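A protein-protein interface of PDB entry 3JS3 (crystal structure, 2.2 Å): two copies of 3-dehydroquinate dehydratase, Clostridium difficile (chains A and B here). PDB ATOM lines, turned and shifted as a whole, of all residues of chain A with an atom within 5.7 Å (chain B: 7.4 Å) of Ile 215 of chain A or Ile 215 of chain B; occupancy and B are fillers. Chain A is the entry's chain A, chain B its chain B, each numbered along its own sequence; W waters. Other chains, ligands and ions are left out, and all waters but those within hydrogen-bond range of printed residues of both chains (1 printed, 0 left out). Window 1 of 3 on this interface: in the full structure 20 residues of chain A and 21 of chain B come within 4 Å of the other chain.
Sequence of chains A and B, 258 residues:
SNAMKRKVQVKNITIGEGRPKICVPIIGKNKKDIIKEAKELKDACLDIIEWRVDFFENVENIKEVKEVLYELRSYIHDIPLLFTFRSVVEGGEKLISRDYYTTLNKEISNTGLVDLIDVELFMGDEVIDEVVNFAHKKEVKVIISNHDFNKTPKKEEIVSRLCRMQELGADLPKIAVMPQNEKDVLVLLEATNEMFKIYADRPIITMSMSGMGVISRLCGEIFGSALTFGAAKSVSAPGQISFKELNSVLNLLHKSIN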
ATOM      1  N   VAL A 185     -28.456   2.853  11.257  1.00  0.00           N
ATOM      2  CA  VAL A 185     -27.254   2.090  11.428  1.00  0.00           C
ATOM      3  C   VAL A 185     -26.226   2.486  10.365  1.00  0.00           C
ATOM      4  O   VAL A 185     -25.046   2.638  10.667  1.00  0.00           O
ATOM      5  CB  VAL A 185     -27.511   0.570  11.361  1.00  0.00           C
ATOM      6  CG1 VAL A 185     -26.156  -0.193  11.437  1.00  0.00           C
ATOM      7  CG2 VAL A 185     -28.455   0.143  12.488  1.00  0.00           C
ATOM      8  N   LEU A 189     -22.337   4.267  10.421  1.00  0.00           N
ATOM      9  CA  LEU A 189     -21.208   3.789   9.647  1.00  0.00           C
ATOM     10  C   LEU A 189     -20.708   4.871   8.689  1.00  0.00           C
ATOM     11  O   LEU A 189     -19.516   5.070   8.544  1.00  0.00           O
ATOM     12  CB  LEU A 189     -21.572   2.528   8.880  1.00  0.00           C
ATOM     13  CG  LEU A 189     -21.847   1.309   9.738  1.00  0.00           C
ATOM     14  CD1 LEU A 189     -22.191   0.146   8.851  1.00  0.00           C
ATOM     15  CD2 LEU A 189     -20.612   0.973  10.625  1.00  0.00           C
ATOM     16  N   GLY A 211     -29.443  -4.933  18.945  1.00  0.00           N
ATOM     17  CA  GLY A 211     -29.334  -6.009  17.967  1.00  0.00           C
ATOM     18  C   GLY A 211     -29.302  -5.512  16.530  1.00  0.00           C
ATOM     19  O   GLY A 211     -28.564  -6.041  15.691  1.00  0.00           O
ATOM     20  N   MET A 212     -30.065  -4.467  16.249  1.00  0.00           N
ATOM     21  CA  MET A 212     -30.126  -3.916  14.891  1.00  0.00           C
ATOM     22  C   MET A 212     -28.791  -3.347  14.403  1.00  0.00           C
ATOM     23  O   MET A 212     -28.438  -3.478  13.240  1.00  0.00           O
ATOM     24  CB  MET A 212     -31.225  -2.845  14.827  1.00  0.00           C
ATOM     25  CG  MET A 212     -31.463  -2.261  13.481  1.00  0.00           C
ATOM     26  SD  MET A 212     -32.912  -1.181  13.445  1.00  0.00           S
ATOM     27  CE  MET A 212     -34.273  -2.322  13.787  1.00  0.00           C
ATOM     28  N   GLY A 213     -28.046  -2.727  15.292  1.00  0.00           N
ATOM     29  CA  GLY A 213     -26.774  -2.125  14.916  1.00  0.00           C
ATOM     30  C   GLY A 213     -25.521  -2.943  15.166  1.00  0.00           C
ATOM     31  O   GLY A 213     -24.430  -2.411  15.039  1.00  0.00           O
ATOM     32  N   VAL A 214     -25.675  -4.226  15.498  1.00  0.00           N
ATOM     33  CA  VAL A 214     -24.550  -5.109  15.785  1.00  0.00           C
ATOM     34  C   VAL A 214     -23.496  -5.138  14.690  1.00  0.00           C
ATOM     35  O   VAL A 214     -22.320  -5.367  14.966  1.00  0.00           O
ATOM     36  CB  VAL A 214     -25.017  -6.553  16.054  1.00  0.00           C
ATOM     37  CG1 VAL A 214     -23.817  -7.523  16.134  1.00  0.00           C
ATOM     38  CG2 VAL A 214     -25.806  -6.615  17.343  1.00  0.00           C
ATOM     39  N   ILE A 215     -23.896  -4.930  13.447  1.00  0.00           N
ATOM     40  CA  ILE A 215     -22.927  -4.921  12.376  1.00  0.00           C
ATOM     41  C   ILE A 215     -21.839  -3.891  12.652  1.00  0.00           C
ATOM     42  O   ILE A 215     -20.689  -4.080  12.236  1.00  0.00           O
ATOM     43  CB  ILE A 215     -23.581  -4.549  11.006  1.00  0.00           C
ATOM     44  CG1 ILE A 215     -22.546  -4.611   9.864  1.00  0.00           C
ATOM     45  CG2 ILE A 215     -24.165  -3.155  11.052  1.00  0.00           C
ATOM     46  CD1 ILE A 215     -23.095  -4.083   8.496  1.00  0.00           C
ATOM     47  N   SER A 216     -22.197  -2.786  13.327  1.00  0.00           N
ATOM     48  CA  SER A 216     -21.227  -1.708  13.591  1.00  0.00           C
ATOM     49  C   SER A 216     -20.111  -2.131  14.536  1.00  0.00           C
ATOM     50  O   SER A 216     -19.143  -1.413  14.682  1.00  0.00           O
ATOM     51  CB  SER A 216     -21.901  -0.471  14.177  1.00  0.00           C
ATOM     52  OG  SER A 216     -22.435  -0.687  15.483  1.00  0.00           O
ATOM     53  N   ARG A 217     -20.295  -3.260  15.205  1.00  0.00           N
ATOM     54  CA  ARG A 217     -19.354  -3.761  16.180  1.00  0.00           C
ATOM     55  C   ARG A 217     -18.368  -4.734  15.541  1.00  0.00           C
ATOM     56  O   ARG A 217     -17.309  -5.027  16.101  1.00  0.00           O
ATOM     57  CB  ARG A 217     -20.107  -4.460  17.334  1.00  0.00           C
ATOM     58  CG  ARG A 217     -21.049  -3.547  18.118  1.00  0.00           C
ATOM     59  CD  ARG A 217     -21.642  -4.272  19.303  1.00  0.00           C
ATOM     60  NE  ARG A 217     -22.507  -3.451  20.164  1.00  0.00           N
ATOM     61  CZ  ARG A 217     -22.085  -2.650  21.151  1.00  0.00           C
ATOM     62  NH1 ARG A 217     -20.794  -2.498  21.415  1.00  0.00           N
ATOM     63  NH2 ARG A 217     -22.964  -1.969  21.875  1.00  0.00           N
ATOM     64  N   LEU A 218     -18.710  -5.183  14.345  1.00  0.00           N
ATOM     65  CA  LEU A 218     -17.925  -6.141  13.622  1.00  0.00           C
ATOM     66  C   LEU A 218     -17.101  -5.614  12.484  1.00  0.00           C
ATOM     67  O   LEU A 218     -16.085  -6.191  12.145  1.00  0.00           O
ATOM     68  CB  LEU A 218     -18.888  -7.151  12.989  1.00  0.00           C
ATOM     69  CG  LEU A 218     -19.919  -7.765  13.927  1.00  0.00           C
ATOM     70  CD1 LEU A 218     -20.843  -8.682  13.129  1.00  0.00           C
ATOM     71  CD2 LEU A 218     -19.216  -8.490  15.074  1.00  0.00           C
ATOM     72  N   CYS A 219     -17.548  -4.537  11.864  1.00  0.00           N
ATOM     73  CA  CYS A 219     -16.922  -4.086  10.630  1.00  0.00           C
ATOM     74  C   CYS A 219     -15.995  -2.916  10.810  1.00  0.00           C
ATOM     75  O   CYS A 219     -15.778  -2.153   9.880  1.00  0.00           O
ATOM     76  CB  CYS A 219     -18.035  -3.690   9.652  1.00  0.00           C
ATOM     77  SG  CYS A 219     -18.805  -2.111  10.087  1.00  0.00           S
ATOM     78  N   GLY A 220     -15.430  -2.766  11.987  1.00  0.00           N
ATOM     79  CA  GLY A 220     -14.578  -1.632  12.241  1.00  0.00           C
ATOM     80  C   GLY A 220     -13.393  -1.546  11.308  1.00  0.00           C
ATOM     81  O   GLY A 220     -12.951  -0.446  10.965  1.00  0.00           O
ATOM     82  N   PHE A 223     -14.712   0.160   8.092  1.00  0.00           N
ATOM     83  CA  PHE A 223     -15.314   1.465   8.291  1.00  0.00           C
ATOM     84  C   PHE A 223     -14.606   2.502   9.164  1.00  0.00           C
ATOM     85  O   PHE A 223     -14.871   3.705   8.997  1.00  0.00           O
ATOM     86  CB  PHE A 223     -16.788   1.306   8.615  1.00  0.00           C
ATOM     87  CG  PHE A 223     -17.577   0.760   7.465  1.00  0.00           C
ATOM     88  CD1 PHE A 223     -18.047   1.596   6.478  1.00  0.00           C
ATOM     89  CD2 PHE A 223     -17.799  -0.597   7.336  1.00  0.00           C
ATOM     90  CE1 PHE A 223     -18.760   1.099   5.399  1.00  0.00           C
ATOM     91  CE2 PHE A 223     -18.497  -1.104   6.252  1.00  0.00           C
ATOM     92  CZ  PHE A 223     -18.980  -0.248   5.278  1.00  0.00           C
ATOM     93  N   LEU A 253     -12.863 -11.452   9.230  1.00  0.00           N
ATOM     94  CA  LEU A 253     -12.890 -10.253   8.378  1.00  0.00           C
ATOM     95  C   LEU A 253     -11.503  -9.652   8.126  1.00  0.00           C
ATOM     96  O   LEU A 253     -11.328  -8.864   7.196  1.00  0.00           O
ATOM     97  CB  LEU A 253     -13.794  -9.185   8.964  1.00  0.00           C
ATOM     98  CG  LEU A 253     -15.276  -9.521   9.157  1.00  0.00           C
ATOM     99  CD1 LEU A 253     -15.957  -8.294   9.720  1.00  0.00           C
ATOM    100  CD2 LEU A 253     -15.939  -9.960   7.866  1.00  0.00           C
ATOM    101  N   VAL B 185     -20.561   0.575  -0.268  1.00  0.00           N
ATOM    102  CA  VAL B 185     -21.047  -0.599   0.436  1.00  0.00           C
ATOM    103  C   VAL B 185     -22.321  -0.264   1.176  1.00  0.00           C
ATOM    104  O   VAL B 185     -23.263  -1.078   1.230  1.00  0.00           O
ATOM    105  CB  VAL B 185     -20.004  -1.162   1.426  1.00  0.00           C
ATOM    106  CG1 VAL B 185     -20.562  -2.398   2.143  1.00  0.00           C
ATOM    107  CG2 VAL B 185     -18.703  -1.503   0.683  1.00  0.00           C
ATOM    108  N   LEU B 186     -22.376   0.950   1.708  1.00  0.00           N
ATOM    109  CA  LEU B 186     -23.557   1.404   2.452  1.00  0.00           C
ATOM    110  C   LEU B 186     -24.709   1.672   1.481  1.00  0.00           C
ATOM    111  O   LEU B 186     -25.873   1.479   1.822  1.00  0.00           O
ATOM    112  CB  LEU B 186     -23.234   2.644   3.282  1.00  0.00           C
ATOM    113  CG  LEU B 186     -22.059   2.454   4.262  1.00  0.00           C
ATOM    114  CD1 LEU B 186     -21.614   3.772   4.930  1.00  0.00           C
ATOM    115  CD2 LEU B 186     -22.407   1.408   5.281  1.00  0.00           C
ATOM    116  N   LEU B 189     -26.415  -1.591   0.881  1.00  0.00           N
ATOM    117  CA  LEU B 189     -27.241  -1.956   2.011  1.00  0.00           C
ATOM    118  C   LEU B 189     -28.486  -1.091   2.098  1.00  0.00           C
ATOM    119  O   LEU B 189     -29.562  -1.565   2.431  1.00  0.00           O
ATOM    120  CB  LEU B 189     -26.445  -1.879   3.310  1.00  0.00           C
ATOM    121  CG  LEU B 189     -25.323  -2.918   3.473  1.00  0.00           C
ATOM    122  CD1 LEU B 189     -24.550  -2.655   4.745  1.00  0.00           C
ATOM    123  CD2 LEU B 189     -25.903  -4.347   3.462  1.00  0.00           C
ATOM    124  N   SER B 208     -22.503  -6.717  -1.974  1.00  0.00           N
ATOM    125  CA  SER B 208     -21.475  -5.806  -2.413  1.00  0.00           C
ATOM    126  C   SER B 208     -20.261  -6.712  -2.463  1.00  0.00           C
ATOM    127  O   SER B 208     -19.909  -7.310  -1.439  1.00  0.00           O
ATOM    128  CB  SER B 208     -21.286  -4.682  -1.393  1.00  0.00           C
ATOM    129  OG  SER B 208     -20.264  -3.807  -1.812  1.00  0.00           O
ATOM    130  N   SER B 210     -16.118  -8.062  -3.290  1.00  0.00           N
ATOM    131  CA  SER B 210     -14.770  -7.773  -2.784  1.00  0.00           C
ATOM    132  C   SER B 210     -14.706  -7.792  -1.241  1.00  0.00           C
ATOM    133  O   SER B 210     -15.733  -7.829  -0.542  1.00  0.00           O
ATOM    134  CB  SER B 210     -14.222  -6.436  -3.324  1.00  0.00           C
ATOM    135  OG  SER B 210     -14.803  -5.343  -2.654  1.00  0.00           O
ATOM    136  N   GLY B 211     -13.488  -7.756  -0.714  1.00  0.00           N
ATOM    137  CA  GLY B 211     -13.279  -7.775   0.741  1.00  0.00           C
ATOM    138  C   GLY B 211     -13.992  -6.639   1.428  1.00  0.00           C
ATOM    139  O   GLY B 211     -14.578  -6.806   2.502  1.00  0.00           O
ATOM    140  N   MET B 212     -13.947  -5.478   0.787  1.00  0.00           N
ATOM    141  CA  MET B 212     -14.584  -4.272   1.291  1.00  0.00           C
ATOM    142  C   MET B 212     -16.091  -4.427   1.472  1.00  0.00           C
ATOM    143  O   MET B 212     -16.689  -3.797   2.364  1.00  0.00           O
ATOM    144  CB  MET B 212     -14.295  -3.092   0.334  1.00  0.00           C
ATOM    145  CG  MET B 212     -14.805  -1.793   0.854  1.00  0.00           C
ATOM    146  SD  MET B 212     -14.360  -0.361  -0.133  1.00  0.00           S
ATOM    147  CE  MET B 212     -12.582  -0.299   0.060  1.00  0.00           C
ATOM    148  N   GLY B 213     -16.710  -5.241   0.618  1.00  0.00           N
ATOM    149  CA  GLY B 213     -18.161  -5.478   0.688  1.00  0.00           C
ATOM    150  C   GLY B 213     -18.593  -6.713   1.474  1.00  0.00           C
ATOM    151  O   GLY B 213     -19.805  -6.971   1.615  1.00  0.00           O
ATOM    152  N   VAL B 214     -17.622  -7.466   1.997  1.00  0.00           N
ATOM    153  CA  VAL B 214     -17.907  -8.727   2.701  1.00  0.00           C
ATOM    154  C   VAL B 214     -18.968  -8.637   3.775  1.00  0.00           C
ATOM    155  O   VAL B 214     -19.714  -9.599   3.992  1.00  0.00           O
ATOM    156  CB  VAL B 214     -16.640  -9.386   3.293  1.00  0.00           C
ATOM    157  CG1 VAL B 214     -17.020 -10.590   4.132  1.00  0.00           C
ATOM    158  CG2 VAL B 214     -15.722  -9.842   2.181  1.00  0.00           C
ATOM    159  N   ILE B 215     -19.069  -7.476   4.411  1.00  0.00           N
ATOM    160  CA  ILE B 215     -20.045  -7.262   5.453  1.00  0.00           C
ATOM    161  C   ILE B 215     -21.491  -7.449   4.950  1.00  0.00           C
ATOM    162  O   ILE B 215     -22.398  -7.793   5.740  1.00  0.00           O
ATOM    163  CB  ILE B 215     -19.887  -5.853   6.046  1.00  0.00           C
ATOM    164  CG1 ILE B 215     -20.471  -5.788   7.463  1.00  0.00           C
ATOM    165  CG2 ILE B 215     -20.465  -4.798   5.093  1.00  0.00           C
ATOM    166  CD1 ILE B 215     -19.664  -6.594   8.522  1.00  0.00           C
ATOM    167  N   SER B 216     -21.726  -7.237   3.660  1.00  0.00           N
ATOM    168  CA  SER B 216     -23.063  -7.412   3.083  1.00  0.00           C
ATOM    169  C   SER B 216     -23.472  -8.887   2.924  1.00  0.00           C
ATOM    170  O   SER B 216     -24.620  -9.187   2.609  1.00  0.00           O
ATOM    171  CB  SER B 216     -23.173  -6.718   1.728  1.00  0.00           C
ATOM    172  OG  SER B 216     -22.273  -7.270   0.783  1.00  0.00           O
ATOM    173  N   ARG B 217     -22.525  -9.792   3.088  1.00  0.00           N
ATOM    174  CA  ARG B 217     -22.791 -11.217   3.009  1.00  0.00           C
ATOM    175  C   ARG B 217     -23.160 -11.768   4.359  1.00  0.00           C
ATOM    176  O   ARG B 217     -23.661 -12.879   4.475  1.00  0.00           O
ATOM    177  CB  ARG B 217     -21.551 -11.939   2.496  1.00  0.00           C
ATOM    178  CG  ARG B 217     -21.127 -11.481   1.110  1.00  0.00           C
ATOM    179  CD  ARG B 217     -20.012 -12.356   0.558  1.00  0.00           C
ATOM    180  NE  ARG B 217     -19.530 -11.898  -0.749  1.00  0.00           N
ATOM    181  CZ  ARG B 217     -20.078 -12.209  -1.919  1.00  0.00           C
ATOM    182  NH1 ARG B 217     -19.538 -11.738  -3.039  1.00  0.00           N
ATOM    183  NH2 ARG B 217     -21.166 -12.980  -1.987  1.00  0.00           N
ATOM    184  N   LEU B 218     -22.929 -10.972   5.392  1.00  0.00           N
ATOM    185  CA  LEU B 218     -23.159 -11.402   6.735  1.00  0.00           C
ATOM    186  C   LEU B 218     -24.401 -10.845   7.441  1.00  0.00           C
ATOM    187  O   LEU B 218     -24.895 -11.482   8.376  1.00  0.00           O
ATOM    188  CB  LEU B 218     -21.957 -10.992   7.571  1.00  0.00           C
ATOM    189  CG  LEU B 218     -20.559 -11.385   7.089  1.00  0.00           C
ATOM    190  CD1 LEU B 218     -19.529 -10.841   8.032  1.00  0.00           C
ATOM    191  CD2 LEU B 218     -20.396 -12.879   6.969  1.00  0.00           C
ATOM    192  N   CYS B 219     -24.919  -9.690   7.001  1.00  0.00           N
ATOM    193  CA  CYS B 219     -26.047  -9.040   7.684  1.00  0.00           C
ATOM    194  C   CYS B 219     -27.368  -8.962   6.922  1.00  0.00           C
ATOM    195  O   CYS B 219     -28.145  -8.039   7.125  1.00  0.00           O
ATOM    196  CB  CYS B 219     -25.641  -7.624   8.069  1.00  0.00           C
ATOM    197  SG  CYS B 219     -25.368  -6.562   6.663  1.00  0.00           S
ATOM    198  N   GLY B 220     -27.650  -9.940   6.078  1.00  0.00           N
ATOM    199  CA  GLY B 220     -28.888  -9.937   5.302  1.00  0.00           C
ATOM    200  C   GLY B 220     -30.146  -9.966   6.160  1.00  0.00           C
ATOM    201  O   GLY B 220     -31.190  -9.457   5.760  1.00  0.00           O
ATOM    202  N   ILE B 222     -30.807  -8.370   8.922  1.00  0.00           N
ATOM    203  CA  ILE B 222     -31.172  -7.011   9.284  1.00  0.00           C
ATOM    204  C   ILE B 222     -31.543  -6.144   8.097  1.00  0.00           C
ATOM    205  O   ILE B 222     -32.533  -5.443   8.145  1.00  0.00           O
ATOM    206  CB  ILE B 222     -30.031  -6.276  10.055  1.00  0.00           C
ATOM    207  CG1 ILE B 222     -30.081  -6.585  11.559  1.00  0.00           C
ATOM    208  CG2 ILE B 222     -30.191  -4.769   9.907  1.00  0.00           C
ATOM    209  CD1 ILE B 222     -30.042  -8.055  11.930  1.00  0.00           C
ATOM    210  N   PHE B 223     -30.740  -6.180   7.037  1.00  0.00           N
ATOM    211  CA  PHE B 223     -30.961  -5.298   5.892  1.00  0.00           C
ATOM    212  C   PHE B 223     -31.851  -5.833   4.772  1.00  0.00           C
ATOM    213  O   PHE B 223     -32.283  -5.065   3.933  1.00  0.00           O
ATOM    214  CB  PHE B 223     -29.636  -4.762   5.375  1.00  0.00           C
ATOM    215  CG  PHE B 223     -28.892  -3.931   6.395  1.00  0.00           C
ATOM    216  CD1 PHE B 223     -29.227  -2.601   6.592  1.00  0.00           C
ATOM    217  CD2 PHE B 223     -27.887  -4.490   7.163  1.00  0.00           C
ATOM    218  CE1 PHE B 223     -28.575  -1.834   7.523  1.00  0.00           C
ATOM    219  CE2 PHE B 223     -27.222  -3.745   8.103  1.00  0.00           C
ATOM    220  CZ  PHE B 223     -27.564  -2.406   8.292  1.00  0.00           C
ATOM    221  N   GLY B 239     -14.893 -11.680  -2.870  1.00  0.00           N
ATOM    222  CA  GLY B 239     -15.360 -11.386  -1.523  1.00  0.00           C
ATOM    223  C   GLY B 239     -16.154 -12.482  -0.858  1.00  0.00           C
ATOM    224  O   GLY B 239     -16.913 -12.216   0.059  1.00  0.00           O
ATOM    225  N   ILE B 241     -16.638 -15.706   1.592  1.00  0.00           N
ATOM    226  CA  ILE B 241     -16.119 -16.299   2.815  1.00  0.00           C
ATOM    227  C   ILE B 241     -16.412 -17.798   2.727  1.00  0.00           C
ATOM    228  O   ILE B 241     -17.371 -18.191   2.042  1.00  0.00           O
ATOM    229  CB  ILE B 241     -16.914 -15.785   4.034  1.00  0.00           C
ATOM    230  CG1 ILE B 241     -16.873 -14.276   4.118  1.00  0.00           C
ATOM    231  CG2 ILE B 241     -16.379 -16.371   5.320  1.00  0.00           C
ATOM    232  CD1 ILE B 241     -17.723 -13.755   5.213  1.00  0.00           C
ATOM    233  N   LEU B 253     -25.669 -13.999  14.516  1.00  0.00           N
ATOM    234  CA  LEU B 253     -26.442 -12.751  14.323  1.00  0.00           C
ATOM    235  C   LEU B 253     -27.959 -12.958  14.342  1.00  0.00           C
ATOM    236  O   LEU B 253     -28.714 -12.006  14.593  1.00  0.00           O
ATOM    237  CB  LEU B 253     -26.045 -12.035  13.016  1.00  0.00           C
ATOM    238  CG  LEU B 253     -24.701 -11.292  13.004  1.00  0.00           C
ATOM    239  CD1 LEU B 253     -24.350 -10.726  11.623  1.00  0.00           C
ATOM    240  CD2 LEU B 253     -24.718 -10.172  14.019  1.00  0.00           C
ATOM    241  N   SER B 256     -29.718 -12.355  18.192  1.00  0.00           N
ATOM    242  CA  SER B 256     -29.038 -11.121  18.587  1.00  0.00           C
ATOM    243  C   SER B 256     -30.015  -9.955  18.742  1.00  0.00           C
ATOM    244  O   SER B 256     -30.812  -9.675  17.844  1.00  0.00           O
ATOM    245  CB  SER B 256     -27.970 -10.790  17.529  1.00  0.00           C
ATOM    246  OG  SER B 256     -27.138  -9.719  17.907  1.00  0.00           O
HETATM  247  O   HOH W   1     -28.205  -8.569  14.857  1.00  0.00           O
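The backbone carbonyl oxygen (O) of Ile 215 of chain B lies within hydrogen-bond range of the side-chain sulfur (SG) of Cys 219 of chain B, at 3.3 Å. The backbone carbonyl oxygen of Ile 215 of chain A is in hydrogen-bond range of the side-chain sulfur of Cys 219 of chain A, 3.5 Å away.
Water W1 lies within hydrogen-bond range of the backbone carbonyl oxygen (O) of Gly 211 of chain A (2.7 Å), the side-chain hydroxyl (OG) of Ser 256 of chain B (3.4 Å) and the backbone carbonyl oxygen (O) of Leu 253 of chain B (3.5 Å).
Printed residues of chain B within 4 Å of Val 214 of chain A: Leu 253 and Ser 256. Of the printed residues of chain B, Ile 215 of chain A touches Ile 215 and Cys 219. Met 212 of chain B touches none of the printed residues of chain A. Ile 215 of chain B touches just these residues of chain A: Ile 215 and Cys 219. Printed residues of chain A within 4 Å of Cys 219 of chain B: Ile 215 (3.8 Å). Gly 220 of chain B touches none of the printed residues of chain A. Of the printed residues of chain A, Leu 253 of chain B touches Val 214. The nearest printed residue of chain B that does not touch Met 212 of chain A is Phe 223 of chain B (5.1 Å).
Val 214 of chain A touches Leu 253 of chain B, and with the chains exchanged Leu 253 of chain A touches Val 214 of chain B. Ile 215 of chain B touches its own counterpart, Ile 215 of chain A. Ile 215 of chain A touches Cys 219 of chain B, and with the chains exchanged Cys 219 of chain A touches Ile 215 of chain B. Leu 253 of chain A touches Leu 218 of chain B, but with the chains exchanged Leu 218 of chain A does not touch Leu 253 of chain B (4.2 Å).
Among the printed residues, merely in contact across the chains: Leu 189 of chain A with Leu 186 of chain B (3.8 Å), Gly 211 of chain A with Ser 256 of chain B (3.95 Å), Met 212 of chain A with Ile 222 of chain B (3.9 Å), Val 214 of chain A with Leu 253 of chain B (3.5 Å), Val 214 of chain A with Ser 256 of chain B (3.4 Å), Ile 215 of chain A with Ile 215 of chain B (3.3 Å), Ile 215 of chain A with Cys 219 of chain B (3.8 Å), Cys 219 of chain A with Ile 215 of chain B (3.5 Å), Phe 223 of chain A with Leu 186 of chain B (3.7 Å), Leu 253 of chain A with Val 214 of chain B (3.9 Å) and Leu 253 of chain A with Leu 218 of chain B (3.7 Å).
Of the 21 printed residues of chain B, 8 touch a printed residue of chain A. Hydrophobic or aromatic side chains of chain A that line the printed part of chain B: Leu 189, Val 214, Ile 215, Phe 223 and Leu 253. Among the printed residues, 11 pairs touch across the chains.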
